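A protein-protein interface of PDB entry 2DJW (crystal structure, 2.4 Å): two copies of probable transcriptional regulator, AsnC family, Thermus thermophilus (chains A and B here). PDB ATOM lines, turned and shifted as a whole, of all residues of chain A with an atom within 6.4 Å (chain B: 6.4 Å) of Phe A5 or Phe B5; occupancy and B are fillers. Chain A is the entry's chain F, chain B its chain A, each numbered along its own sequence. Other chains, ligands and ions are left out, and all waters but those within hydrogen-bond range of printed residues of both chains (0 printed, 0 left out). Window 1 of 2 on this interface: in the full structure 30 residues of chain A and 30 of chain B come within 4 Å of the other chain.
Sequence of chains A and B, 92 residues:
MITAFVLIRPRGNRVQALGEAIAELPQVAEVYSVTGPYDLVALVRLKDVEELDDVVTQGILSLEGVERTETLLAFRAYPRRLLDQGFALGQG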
ATOM      1  N   THR A   3     -12.687  29.692   0.899  1.00  0.00           N
ATOM      2  CA  THR A   3     -12.566  28.629  -0.087  1.00  0.00           C
ATOM      3  C   THR A   3     -13.904  28.356  -0.805  1.00  0.00           C
ATOM      4  O   THR A   3     -14.988  28.471  -0.217  1.00  0.00           O
ATOM      5  CB  THR A   3     -11.953  27.364   0.542  1.00  0.00           C
ATOM      6  OG1 THR A   3     -10.628  27.673   1.009  1.00  0.00           O
ATOM      7  CG2 THR A   3     -11.881  26.215  -0.455  1.00  0.00           C
ATOM      8  N   ALA A   4     -13.801  28.055  -2.099  1.00  0.00           N
ATOM      9  CA  ALA A   4     -14.933  27.655  -2.916  1.00  0.00           C
ATOM     10  C   ALA A   4     -14.516  26.506  -3.814  1.00  0.00           C
ATOM     11  O   ALA A   4     -13.341  26.395  -4.191  1.00  0.00           O
ATOM     12  CB  ALA A   4     -15.434  28.822  -3.743  1.00  0.00           C
ATOM     13  N   PHE A   5     -15.475  25.635  -4.117  1.00  0.00           N
ATOM     14  CA  PHE A   5     -15.300  24.559  -5.092  1.00  0.00           C
ATOM     15  C   PHE A   5     -16.185  24.950  -6.265  1.00  0.00           C
ATOM     16  O   PHE A   5     -17.407  25.015  -6.107  1.00  0.00           O
ATOM     17  CB  PHE A   5     -15.733  23.193  -4.504  1.00  0.00           C
ATOM     18  CG  PHE A   5     -14.921  22.778  -3.300  1.00  0.00           C
ATOM     19  CD1 PHE A   5     -13.805  21.960  -3.447  1.00  0.00           C
ATOM     20  CD2 PHE A   5     -15.238  23.264  -2.018  1.00  0.00           C
ATOM     21  CE1 PHE A   5     -13.032  21.608  -2.334  1.00  0.00           C
ATOM     22  CE2 PHE A   5     -14.461  22.922  -0.905  1.00  0.00           C
ATOM     23  CZ  PHE A   5     -13.367  22.084  -1.054  1.00  0.00           C
ATOM     24  N   VAL A   6     -15.560  25.260  -7.408  1.00  0.00           N
ATOM     25  CA  VAL A   6     -16.291  25.628  -8.630  1.00  0.00           C
ATOM     26  C   VAL A   6     -16.352  24.452  -9.592  1.00  0.00           C
ATOM     27  O   VAL A   6     -15.342  23.959 -10.090  1.00  0.00           O
ATOM     28  CB  VAL A   6     -15.746  26.912  -9.351  1.00  0.00           C
ATOM     29  CG1 VAL A   6     -16.771  27.429 -10.339  1.00  0.00           C
ATOM     30  CG2 VAL A   6     -15.426  28.014  -8.350  1.00  0.00           C
ATOM     31  N   LEU A   7     -17.565  23.986  -9.815  1.00  0.00           N
ATOM     32  CA  LEU A   7     -17.807  22.848 -10.668  1.00  0.00           C
ATOM     33  C   LEU A   7     -18.159  23.380 -12.069  1.00  0.00           C
ATOM     34  O   LEU A   7     -19.077  24.174 -12.218  1.00  0.00           O
ATOM     35  CB  LEU A   7     -18.944  22.004 -10.069  1.00  0.00           C
ATOM     36  CG  LEU A   7     -18.684  20.995  -8.922  1.00  0.00           C
ATOM     37  CD1 LEU A   7     -17.807  21.512  -7.791  1.00  0.00           C
ATOM     38  CD2 LEU A   7     -20.027  20.467  -8.365  1.00  0.00           C
ATOM     39  N   GLU A  30      -5.961  25.219  -7.466  1.00  0.00           N
ATOM     40  CA  GLU A  30      -5.922  23.877  -8.043  1.00  0.00           C
ATOM     41  C   GLU A  30      -7.098  23.783  -9.007  1.00  0.00           C
ATOM     42  O   GLU A  30      -8.144  24.366  -8.765  1.00  0.00           O
ATOM     43  CB  GLU A  30      -6.038  22.804  -6.952  1.00  0.00           C
ATOM     44  CG  GLU A  30      -4.817  22.677  -6.031  1.00  0.00           C
ATOM     45  CD  GLU A  30      -5.025  21.713  -4.864  1.00  0.00           C
ATOM     46  OE1 GLU A  30      -5.573  20.606  -5.082  1.00  0.00           O
ATOM     47  OE2 GLU A  30      -4.617  22.062  -3.721  1.00  0.00           O
ATOM     48  N   TYR A  32      -8.836  20.726 -11.843  1.00  0.00           N
ATOM     49  CA  TYR A  32      -8.686  19.338 -12.247  1.00  0.00           C
ATOM     50  C   TYR A  32      -9.720  18.902 -13.226  1.00  0.00           C
ATOM     51  O   TYR A  32     -10.845  19.385 -13.205  1.00  0.00           O
ATOM     52  CB  TYR A  32      -8.807  18.404 -11.039  1.00  0.00           C
ATOM     53  CG  TYR A  32      -7.771  18.619  -9.974  1.00  0.00           C
ATOM     54  CD1 TYR A  32      -6.526  18.005 -10.059  1.00  0.00           C
ATOM     55  CD2 TYR A  32      -8.041  19.424  -8.873  1.00  0.00           C
ATOM     56  CE1 TYR A  32      -5.574  18.192  -9.080  1.00  0.00           C
ATOM     57  CE2 TYR A  32      -7.092  19.628  -7.888  1.00  0.00           C
ATOM     58  CZ  TYR A  32      -5.863  19.007  -7.999  1.00  0.00           C
ATOM     59  OH  TYR A  32      -4.913  19.202  -7.030  1.00  0.00           O
ATOM     60  N   VAL A  34     -11.943  15.809 -13.665  1.00  0.00           N
ATOM     61  CA  VAL A  34     -12.535  14.867 -12.707  1.00  0.00           C
ATOM     62  C   VAL A  34     -13.575  13.925 -13.323  1.00  0.00           C
ATOM     63  O   VAL A  34     -14.200  14.235 -14.355  1.00  0.00           O
ATOM     64  CB  VAL A  34     -13.234  15.607 -11.509  1.00  0.00           C
ATOM     65  CG1 VAL A  34     -12.224  16.353 -10.661  1.00  0.00           C
ATOM     66  CG2 VAL A  34     -14.343  16.547 -12.010  1.00  0.00           C
ATOM     67  N   VAL A  41     -13.219  20.739 -11.973  1.00  0.00           N
ATOM     68  CA  VAL A  41     -13.445  21.365 -10.677  1.00  0.00           C
ATOM     69  C   VAL A  41     -12.308  22.346 -10.449  1.00  0.00           C
ATOM     70  O   VAL A  41     -11.145  21.970 -10.616  1.00  0.00           O
ATOM     71  CB  VAL A  41     -13.442  20.331  -9.500  1.00  0.00           C
ATOM     72  CG1 VAL A  41     -13.716  21.029  -8.171  1.00  0.00           C
ATOM     73  CG2 VAL A  41     -14.477  19.232  -9.724  1.00  0.00           C
ATOM     74  N   ALA A  42     -12.632  23.586 -10.072  1.00  0.00           N
ATOM     75  CA  ALA A  42     -11.595  24.498  -9.581  1.00  0.00           C
ATOM     76  C   ALA A  42     -11.644  24.726  -8.069  1.00  0.00           C
ATOM     77  O   ALA A  42     -12.659  25.185  -7.552  1.00  0.00           O
ATOM     78  CB  ALA A  42     -11.625  25.863 -10.336  1.00  0.00           C
ATOM     79  N   LEU A  43     -10.539  24.433  -7.382  1.00  0.00           N
ATOM     80  CA  LEU A  43     -10.346  24.858  -5.998  1.00  0.00           C
ATOM     81  C   LEU A  43      -9.846  26.310  -5.976  1.00  0.00           C
ATOM     82  O   LEU A  43      -8.713  26.591  -6.386  1.00  0.00           O
ATOM     83  CB  LEU A  43      -9.368  23.930  -5.272  1.00  0.00           C
ATOM     84  CG  LEU A  43      -9.031  24.182  -3.791  1.00  0.00           C
ATOM     85  CD1 LEU A  43     -10.273  24.124  -2.920  1.00  0.00           C
ATOM     86  CD2 LEU A  43      -7.987  23.185  -3.259  1.00  0.00           C
ATOM     87  N   VAL A  44     -10.710  27.212  -5.501  1.00  0.00           N
ATOM     88  CA  VAL A  44     -10.491  28.648  -5.534  1.00  0.00           C
ATOM     89  C   VAL A  44     -10.271  29.180  -4.100  1.00  0.00           C
ATOM     90  O   VAL A  44     -10.817  28.632  -3.142  1.00  0.00           O
ATOM     91  CB  VAL A  44     -11.691  29.366  -6.264  1.00  0.00           C
ATOM     92  CG1 VAL A  44     -11.486  30.830  -6.357  1.00  0.00           C
ATOM     93  CG2 VAL A  44     -11.863  28.844  -7.689  1.00  0.00           C
ATOM     94  N   GLU A  70     -21.154  25.500 -11.249  1.00  0.00           N
ATOM     95  CA  GLU A  70     -21.801  25.404  -9.929  1.00  0.00           C
ATOM     96  C   GLU A  70     -20.839  25.589  -8.764  1.00  0.00           C
ATOM     97  O   GLU A  70     -19.975  24.760  -8.553  1.00  0.00           O
ATOM     98  CB  GLU A  70     -22.595  24.102  -9.784  1.00  0.00           C
ATOM     99  CG  GLU A  70     -23.723  24.214  -8.777  1.00  0.00           C
ATOM    100  CD  GLU A  70     -24.171  22.876  -8.205  1.00  0.00           C
ATOM    101  OE1 GLU A  70     -24.091  21.845  -8.908  1.00  0.00           O
ATOM    102  OE2 GLU A  70     -24.635  22.861  -7.050  1.00  0.00           O
ATOM    103  N   THR A  71     -20.997  26.684  -8.015  1.00  0.00           N
ATOM    104  CA  THR A  71     -20.077  27.022  -6.924  1.00  0.00           C
ATOM    105  C   THR A  71     -20.561  26.517  -5.559  1.00  0.00           C
ATOM    106  O   THR A  71     -21.677  26.819  -5.114  1.00  0.00           O
ATOM    107  CB  THR A  71     -19.748  28.542  -6.841  1.00  0.00           C
ATOM    108  OG1 THR A  71     -19.134  28.961  -8.053  1.00  0.00           O
ATOM    109  CG2 THR A  71     -18.757  28.849  -5.686  1.00  0.00           C
ATOM    110  N   LEU A  72     -19.686  25.742  -4.924  1.00  0.00           N
ATOM    111  CA  LEU A  72     -19.875  25.272  -3.550  1.00  0.00           C
ATOM    112  C   LEU A  72     -18.963  26.105  -2.663  1.00  0.00           C
ATOM    113  O   LEU A  72     -17.762  25.868  -2.609  1.00  0.00           O
ATOM    114  CB  LEU A  72     -19.518  23.789  -3.446  1.00  0.00           C
ATOM    115  CG  LEU A  72     -20.441  22.662  -3.926  1.00  0.00           C
ATOM    116  CD1 LEU A  72     -21.508  23.010  -4.946  1.00  0.00           C
ATOM    117  CD2 LEU A  72     -19.636  21.475  -4.398  1.00  0.00           C
ATOM    118  N   LEU A  73     -19.530  27.097  -1.991  1.00  0.00           N
ATOM    119  CA  LEU A  73     -18.737  27.983  -1.151  1.00  0.00           C
ATOM    120  C   LEU A  73     -18.643  27.537   0.320  1.00  0.00           C
ATOM    121  O   LEU A  73     -19.647  27.327   0.983  1.00  0.00           O
ATOM    122  CB  LEU A  73     -19.253  29.425  -1.238  1.00  0.00           C
ATOM    123  CG  LEU A  73     -18.298  30.510  -0.723  1.00  0.00           C
ATOM    124  CD1 LEU A  73     -17.163  30.731  -1.661  1.00  0.00           C
ATOM    125  CD2 LEU A  73     -18.995  31.797  -0.584  1.00  0.00           C
ATOM    126  N   ALA A  74     -17.416  27.461   0.811  1.00  0.00           N
ATOM    127  CA  ALA A  74     -17.108  26.958   2.141  1.00  0.00           C
ATOM    128  C   ALA A  74     -17.256  28.067   3.159  1.00  0.00           C
ATOM    129  O   ALA A  74     -16.550  29.087   3.096  1.00  0.00           O
ATOM    130  CB  ALA A  74     -15.682  26.390   2.174  1.00  0.00           C
ATOM    131  N   THR B   3      -5.863  13.242  -6.220  1.00  0.00           N
ATOM    132  CA  THR B   3      -6.843  14.081  -5.554  1.00  0.00           C
ATOM    133  C   THR B   3      -8.293  13.653  -5.876  1.00  0.00           C
ATOM    134  O   THR B   3      -8.602  13.224  -6.995  1.00  0.00           O
ATOM    135  CB  THR B   3      -6.606  15.559  -5.877  1.00  0.00           C
ATOM    136  OG1 THR B   3      -5.335  15.942  -5.341  1.00  0.00           O
ATOM    137  CG2 THR B   3      -7.678  16.449  -5.257  1.00  0.00           C
ATOM    138  N   ALA B   4      -9.152  13.764  -4.862  1.00  0.00           N
ATOM    139  CA  ALA B   4     -10.572  13.503  -4.981  1.00  0.00           C
ATOM    140  C   ALA B   4     -11.339  14.544  -4.172  1.00  0.00           C
ATOM    141  O   ALA B   4     -10.844  15.062  -3.163  1.00  0.00           O
ATOM    142  CB  ALA B   4     -10.888  12.094  -4.491  1.00  0.00           C
ATOM    143  N   PHE B   5     -12.540  14.864  -4.631  1.00  0.00           N
ATOM    144  CA  PHE B   5     -13.423  15.787  -3.926  1.00  0.00           C
ATOM    145  C   PHE B   5     -14.579  14.922  -3.492  1.00  0.00           C
ATOM    146  O   PHE B   5     -15.294  14.397  -4.344  1.00  0.00           O
ATOM    147  CB  PHE B   5     -13.906  16.926  -4.855  1.00  0.00           C
ATOM    148  CG  PHE B   5     -12.780  17.785  -5.387  1.00  0.00           C
ATOM    149  CD1 PHE B   5     -12.393  18.938  -4.718  1.00  0.00           C
ATOM    150  CD2 PHE B   5     -12.067  17.405  -6.534  1.00  0.00           C
ATOM    151  CE1 PHE B   5     -11.325  19.710  -5.188  1.00  0.00           C
ATOM    152  CE2 PHE B   5     -11.005  18.177  -7.003  1.00  0.00           C
ATOM    153  CZ  PHE B   5     -10.634  19.331  -6.343  1.00  0.00           C
ATOM    154  N   VAL B   6     -14.729  14.727  -2.179  1.00  0.00           N
ATOM    155  CA  VAL B   6     -15.826  13.891  -1.654  1.00  0.00           C
ATOM    156  C   VAL B   6     -16.972  14.756  -1.147  1.00  0.00           C
ATOM    157  O   VAL B   6     -16.825  15.564  -0.227  1.00  0.00           O
ATOM    158  CB  VAL B   6     -15.392  12.833  -0.594  1.00  0.00           C
ATOM    159  CG1 VAL B   6     -16.514  11.856  -0.350  1.00  0.00           C
ATOM    160  CG2 VAL B   6     -14.149  12.074  -1.058  1.00  0.00           C
ATOM    161  N   LEU B   7     -18.110  14.597  -1.802  1.00  0.00           N
ATOM    162  CA  LEU B   7     -19.292  15.351  -1.482  1.00  0.00           C
ATOM    163  C   LEU B   7     -20.150  14.517  -0.501  1.00  0.00           C
ATOM    164  O   LEU B   7     -20.581  13.415  -0.822  1.00  0.00           O
ATOM    165  CB  LEU B   7     -20.047  15.656  -2.785  1.00  0.00           C
ATOM    166  CG  LEU B   7     -19.693  16.842  -3.728  1.00  0.00           C
ATOM    167  CD1 LEU B   7     -18.198  17.118  -3.952  1.00  0.00           C
ATOM    168  CD2 LEU B   7     -20.419  16.682  -5.075  1.00  0.00           C
ATOM    169  N   GLU B  30      -8.496  18.816   3.802  1.00  0.00           N
ATOM    170  CA  GLU B  30      -9.382  19.948   4.066  1.00  0.00           C
ATOM    171  C   GLU B  30     -10.786  19.385   4.046  1.00  0.00           C
ATOM    172  O   GLU B  30     -11.072  18.522   3.252  1.00  0.00           O
ATOM    173  CB  GLU B  30      -9.242  21.041   2.989  1.00  0.00           C
ATOM    174  CG  GLU B  30      -7.889  21.776   2.959  1.00  0.00           C
ATOM    175  CD  GLU B  30      -7.728  22.723   1.776  1.00  0.00           C
ATOM    176  OE1 GLU B  30      -8.701  23.455   1.445  1.00  0.00           O
ATOM    177  OE2 GLU B  30      -6.608  22.747   1.190  1.00  0.00           O
ATOM    178  N   TYR B  32     -14.999  20.933   4.710  1.00  0.00           N
ATOM    179  CA  TYR B  32     -15.739  22.153   4.903  1.00  0.00           C
ATOM    180  C   TYR B  32     -17.212  21.902   4.906  1.00  0.00           C
ATOM    181  O   TYR B  32     -17.700  20.977   4.265  1.00  0.00           O
ATOM    182  CB  TYR B  32     -15.467  23.153   3.771  1.00  0.00           C
ATOM    183  CG  TYR B  32     -14.039  23.561   3.608  1.00  0.00           C
ATOM    184  CD1 TYR B  32     -13.512  24.616   4.336  1.00  0.00           C
ATOM    185  CD2 TYR B  32     -13.214  22.894   2.713  1.00  0.00           C
ATOM    186  CE1 TYR B  32     -12.179  24.990   4.191  1.00  0.00           C
ATOM    187  CE2 TYR B  32     -11.886  23.252   2.557  1.00  0.00           C
ATOM    188  CZ  TYR B  32     -11.377  24.304   3.297  1.00  0.00           C
ATOM    189  OH  TYR B  32     -10.060  24.662   3.138  1.00  0.00           O
ATOM    190  N   VAL B  34     -20.255  23.617   3.336  1.00  0.00           N
ATOM    191  CA  VAL B  34     -20.436  24.380   2.099  1.00  0.00           C
ATOM    192  C   VAL B  34     -21.901  24.684   1.793  1.00  0.00           C
ATOM    193  O   VAL B  34     -22.807  23.983   2.258  1.00  0.00           O
ATOM    194  CB  VAL B  34     -19.837  23.639   0.840  1.00  0.00           C
ATOM    195  CG1 VAL B  34     -18.346  23.629   0.874  1.00  0.00           C
ATOM    196  CG2 VAL B  34     -20.411  22.203   0.704  1.00  0.00           C
ATOM    197  N   VAL B  41     -17.903  18.965   2.077  1.00  0.00           N
ATOM    198  CA  VAL B  41     -17.008  18.524   1.001  1.00  0.00           C
ATOM    199  C   VAL B  41     -15.686  18.179   1.642  1.00  0.00           C
ATOM    200  O   VAL B  41     -15.128  19.017   2.362  1.00  0.00           O
ATOM    201  CB  VAL B  41     -16.735  19.639  -0.081  1.00  0.00           C
ATOM    202  CG1 VAL B  41     -15.740  19.147  -1.145  1.00  0.00           C
ATOM    203  CG2 VAL B  41     -18.017  20.078  -0.752  1.00  0.00           C
ATOM    204  N   ALA B  42     -15.170  16.979   1.363  1.00  0.00           N
ATOM    205  CA  ALA B  42     -13.801  16.664   1.752  1.00  0.00           C
ATOM    206  C   ALA B  42     -12.815  16.685   0.581  1.00  0.00           C
ATOM    207  O   ALA B  42     -12.983  15.956  -0.388  1.00  0.00           O
ATOM    208  CB  ALA B  42     -13.723  15.304   2.495  1.00  0.00           C
ATOM    209  N   LEU B  43     -11.777  17.505   0.701  1.00  0.00           N
ATOM    210  CA  LEU B  43     -10.630  17.442  -0.190  1.00  0.00           C
ATOM    211  C   LEU B  43      -9.639  16.401   0.350  1.00  0.00           C
ATOM    212  O   LEU B  43      -8.986  16.621   1.382  1.00  0.00           O
ATOM    213  CB  LEU B  43      -9.962  18.813  -0.309  1.00  0.00           C
ATOM    214  CG  LEU B  43      -8.679  18.916  -1.135  1.00  0.00           C
ATOM    215  CD1 LEU B  43      -8.960  18.584  -2.598  1.00  0.00           C
ATOM    216  CD2 LEU B  43      -8.062  20.314  -1.017  1.00  0.00           C
ATOM    217  N   VAL B  44      -9.551  15.280  -0.369  1.00  0.00           N
ATOM    218  CA  VAL B  44      -8.757  14.124   0.000  1.00  0.00           C
ATOM    219  C   VAL B  44      -7.512  14.013  -0.919  1.00  0.00           C
ATOM    220  O   VAL B  44      -7.528  14.472  -2.067  1.00  0.00           O
ATOM    221  CB  VAL B  44      -9.619  12.810  -0.058  1.00  0.00           C
ATOM    222  CG1 VAL B  44      -8.877  11.654   0.510  1.00  0.00           C
ATOM    223  CG2 VAL B  44     -10.919  12.953   0.739  1.00  0.00           C
ATOM    224  N   GLU B  70     -20.808  11.520  -2.738  1.00  0.00           N
ATOM    225  CA  GLU B  70     -20.435  11.513  -4.165  1.00  0.00           C
ATOM    226  C   GLU B  70     -18.994  11.940  -4.402  1.00  0.00           C
ATOM    227  O   GLU B  70     -18.632  13.048  -4.098  1.00  0.00           O
ATOM    228  CB  GLU B  70     -21.391  12.370  -5.007  1.00  0.00           C
ATOM    229  CG  GLU B  70     -21.559  11.840  -6.416  1.00  0.00           C
ATOM    230  CD  GLU B  70     -21.869  12.914  -7.449  1.00  0.00           C
ATOM    231  OE1 GLU B  70     -22.557  13.895  -7.111  1.00  0.00           O
ATOM    232  OE2 GLU B  70     -21.443  12.752  -8.617  1.00  0.00           O
ATOM    233  N   THR B  71     -18.175  11.044  -4.939  1.00  0.00           N
ATOM    234  CA  THR B  71     -16.745  11.295  -5.107  1.00  0.00           C
ATOM    235  C   THR B  71     -16.402  11.730  -6.538  1.00  0.00           C
ATOM    236  O   THR B  71     -16.724  11.027  -7.519  1.00  0.00           O
ATOM    237  CB  THR B  71     -15.898  10.083  -4.715  1.00  0.00           C
ATOM    238  OG1 THR B  71     -16.196   9.725  -3.369  1.00  0.00           O
ATOM    239  CG2 THR B  71     -14.395  10.391  -4.808  1.00  0.00           C
ATOM    240  N   LEU B  72     -15.756  12.896  -6.614  1.00  0.00           N
ATOM    241  CA  LEU B  72     -15.257  13.465  -7.866  1.00  0.00           C
ATOM    242  C   LEU B  72     -13.759  13.231  -7.883  1.00  0.00           C
ATOM    243  O   LEU B  72     -13.025  13.969  -7.238  1.00  0.00           O
ATOM    244  CB  LEU B  72     -15.563  14.967  -7.934  1.00  0.00           C
ATOM    245  CG  LEU B  72     -16.963  15.511  -8.302  1.00  0.00           C
ATOM    246  CD1 LEU B  72     -18.149  14.605  -8.072  1.00  0.00           C
ATOM    247  CD2 LEU B  72     -17.232  16.868  -7.692  1.00  0.00           C
ATOM    248  N   LEU B  73     -13.306  12.203  -8.599  1.00  0.00           N
ATOM    249  CA  LEU B  73     -11.891  11.872  -8.601  1.00  0.00           C
ATOM    250  C   LEU B  73     -11.080  12.557  -9.715  1.00  0.00           C
ATOM    251  O   LEU B  73     -11.375  12.423 -10.887  1.00  0.00           O
ATOM    252  CB  LEU B  73     -11.675  10.344  -8.608  1.00  0.00           C
ATOM    253  CG  LEU B  73     -10.194   9.943  -8.530  1.00  0.00           C
ATOM    254  CD1 LEU B  73      -9.893   8.928  -7.480  1.00  0.00           C
ATOM    255  CD2 LEU B  73      -9.575   9.512  -9.898  1.00  0.00           C
ATOM    256  N   ALA B  74     -10.032  13.259  -9.327  1.00  0.00           N
ATOM    257  CA  ALA B  74      -9.206  14.034 -10.268  1.00  0.00           C
ATOM    258  C   ALA B  74      -8.170  13.159 -10.950  1.00  0.00           C
ATOM    259  O   ALA B  74      -7.260  12.617 -10.295  1.00  0.00           O
ATOM    260  CB  ALA B  74      -8.525  15.193  -9.550  1.00  0.00           C
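Of the 17 printed residues of chain B, 8 touch a printed residue of chain A.
Printed residues of chain A that touch a printed residue of chain B: Thr A3, Phe A5, Tyr A32, Val A34, Val A41, Leu A43, Leu A73 and Ala A74.
Among the printed residues, 14 pairs touch across the chains.
Among the printed residues, no Asp or Glu carboxylate lies within 4 Å of a Lys or Arg side-chain nitrogen of the other chain.
Phe A5 touches Tyr B32, and with the chains exchanged Tyr A32 touches Phe B5.
Tyr A32 touches Ala B74, and with the chains exchanged Ala A74 touches Tyr B32.
Val A34 touches Leu B73, and with the chains exchanged Leu A73 touches Val B34.
Leu A43 touches its own counterpart, Leu B43.
Of the 14 pairs that touch across the chains among the printed residues, 14 have their exchanged pair printed and touching as well.
Of chain B, only Phe B5, Tyr B32 and Val B41 come within 4 Å of Phe A5.
Printed residues of chain B within 4 Å of Tyr A32: Thr B3, Phe B5 and Ala B74.
Of the printed residues of chain B, Val A34 touches Leu B73 and Ala B74.
Ala B4 touches none of the printed residues of chain A.
Phe B5 touches just these residues of chain A: Phe A5, Tyr A32 and Val A41.
Val B44 touches none of the printed residues of chain A.
The nearest residue of chain B that does not touch Phe A5 is Val B34 (4.3 Å).
The nearest residue of chain A that does not touch Phe B5 is Val A34 (4.3 Å).
The nearest printed residue of chain A that does not touch Thr B3 is Glu A30 (4.7 Å).
OH of Tyr A32 sits at hydrogen-bond distance from OE1 of Glu A30, 2.5 Å away.
O of Thr B3 lies within hydrogen-bond range of N of Ala B74, at 2.7 Å.
O of Thr A3 is in hydrogen-bond range of N of Ala A74 (2.8 Å).
O of Phe A5 sits at hydrogen-bond distance from N of Leu A72, at 2.7 Å.
O of Tyr B32 sits at hydrogen-bond distance from N of Val B41, 3.0 Å away.
OE1 of Glu B30 is in hydrogen-bond range of OH of Tyr B32, 2.5 Å away.
Among the printed residues, pairs that only touch across the chains: Leu A73 with Val B34 (3.2 Å), Val A34 with Leu B73 (3.3 Å), Tyr A32 with Ala B74 (3.5 Å), Ala A74 with Tyr B32 (3.5 Å), Phe A5 with Phe B5 (3.6 Å), Tyr A32 with Phe B5 (3.6 Å), Leu A43 with Leu B43 (3.6 Å), Tyr A32 with Thr B3 (3.7 Å), Thr A3 with Tyr B32 (3.7 Å), Ala A74 with Val B34 (3.8 Å), Phe A5 with Val B41 (3.8 Å), Val A34 with Ala B74 (3.8 Å), Phe A5 with Tyr B32 (3.8 Å) and Val A41 with Phe B5 (3.97 Å).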
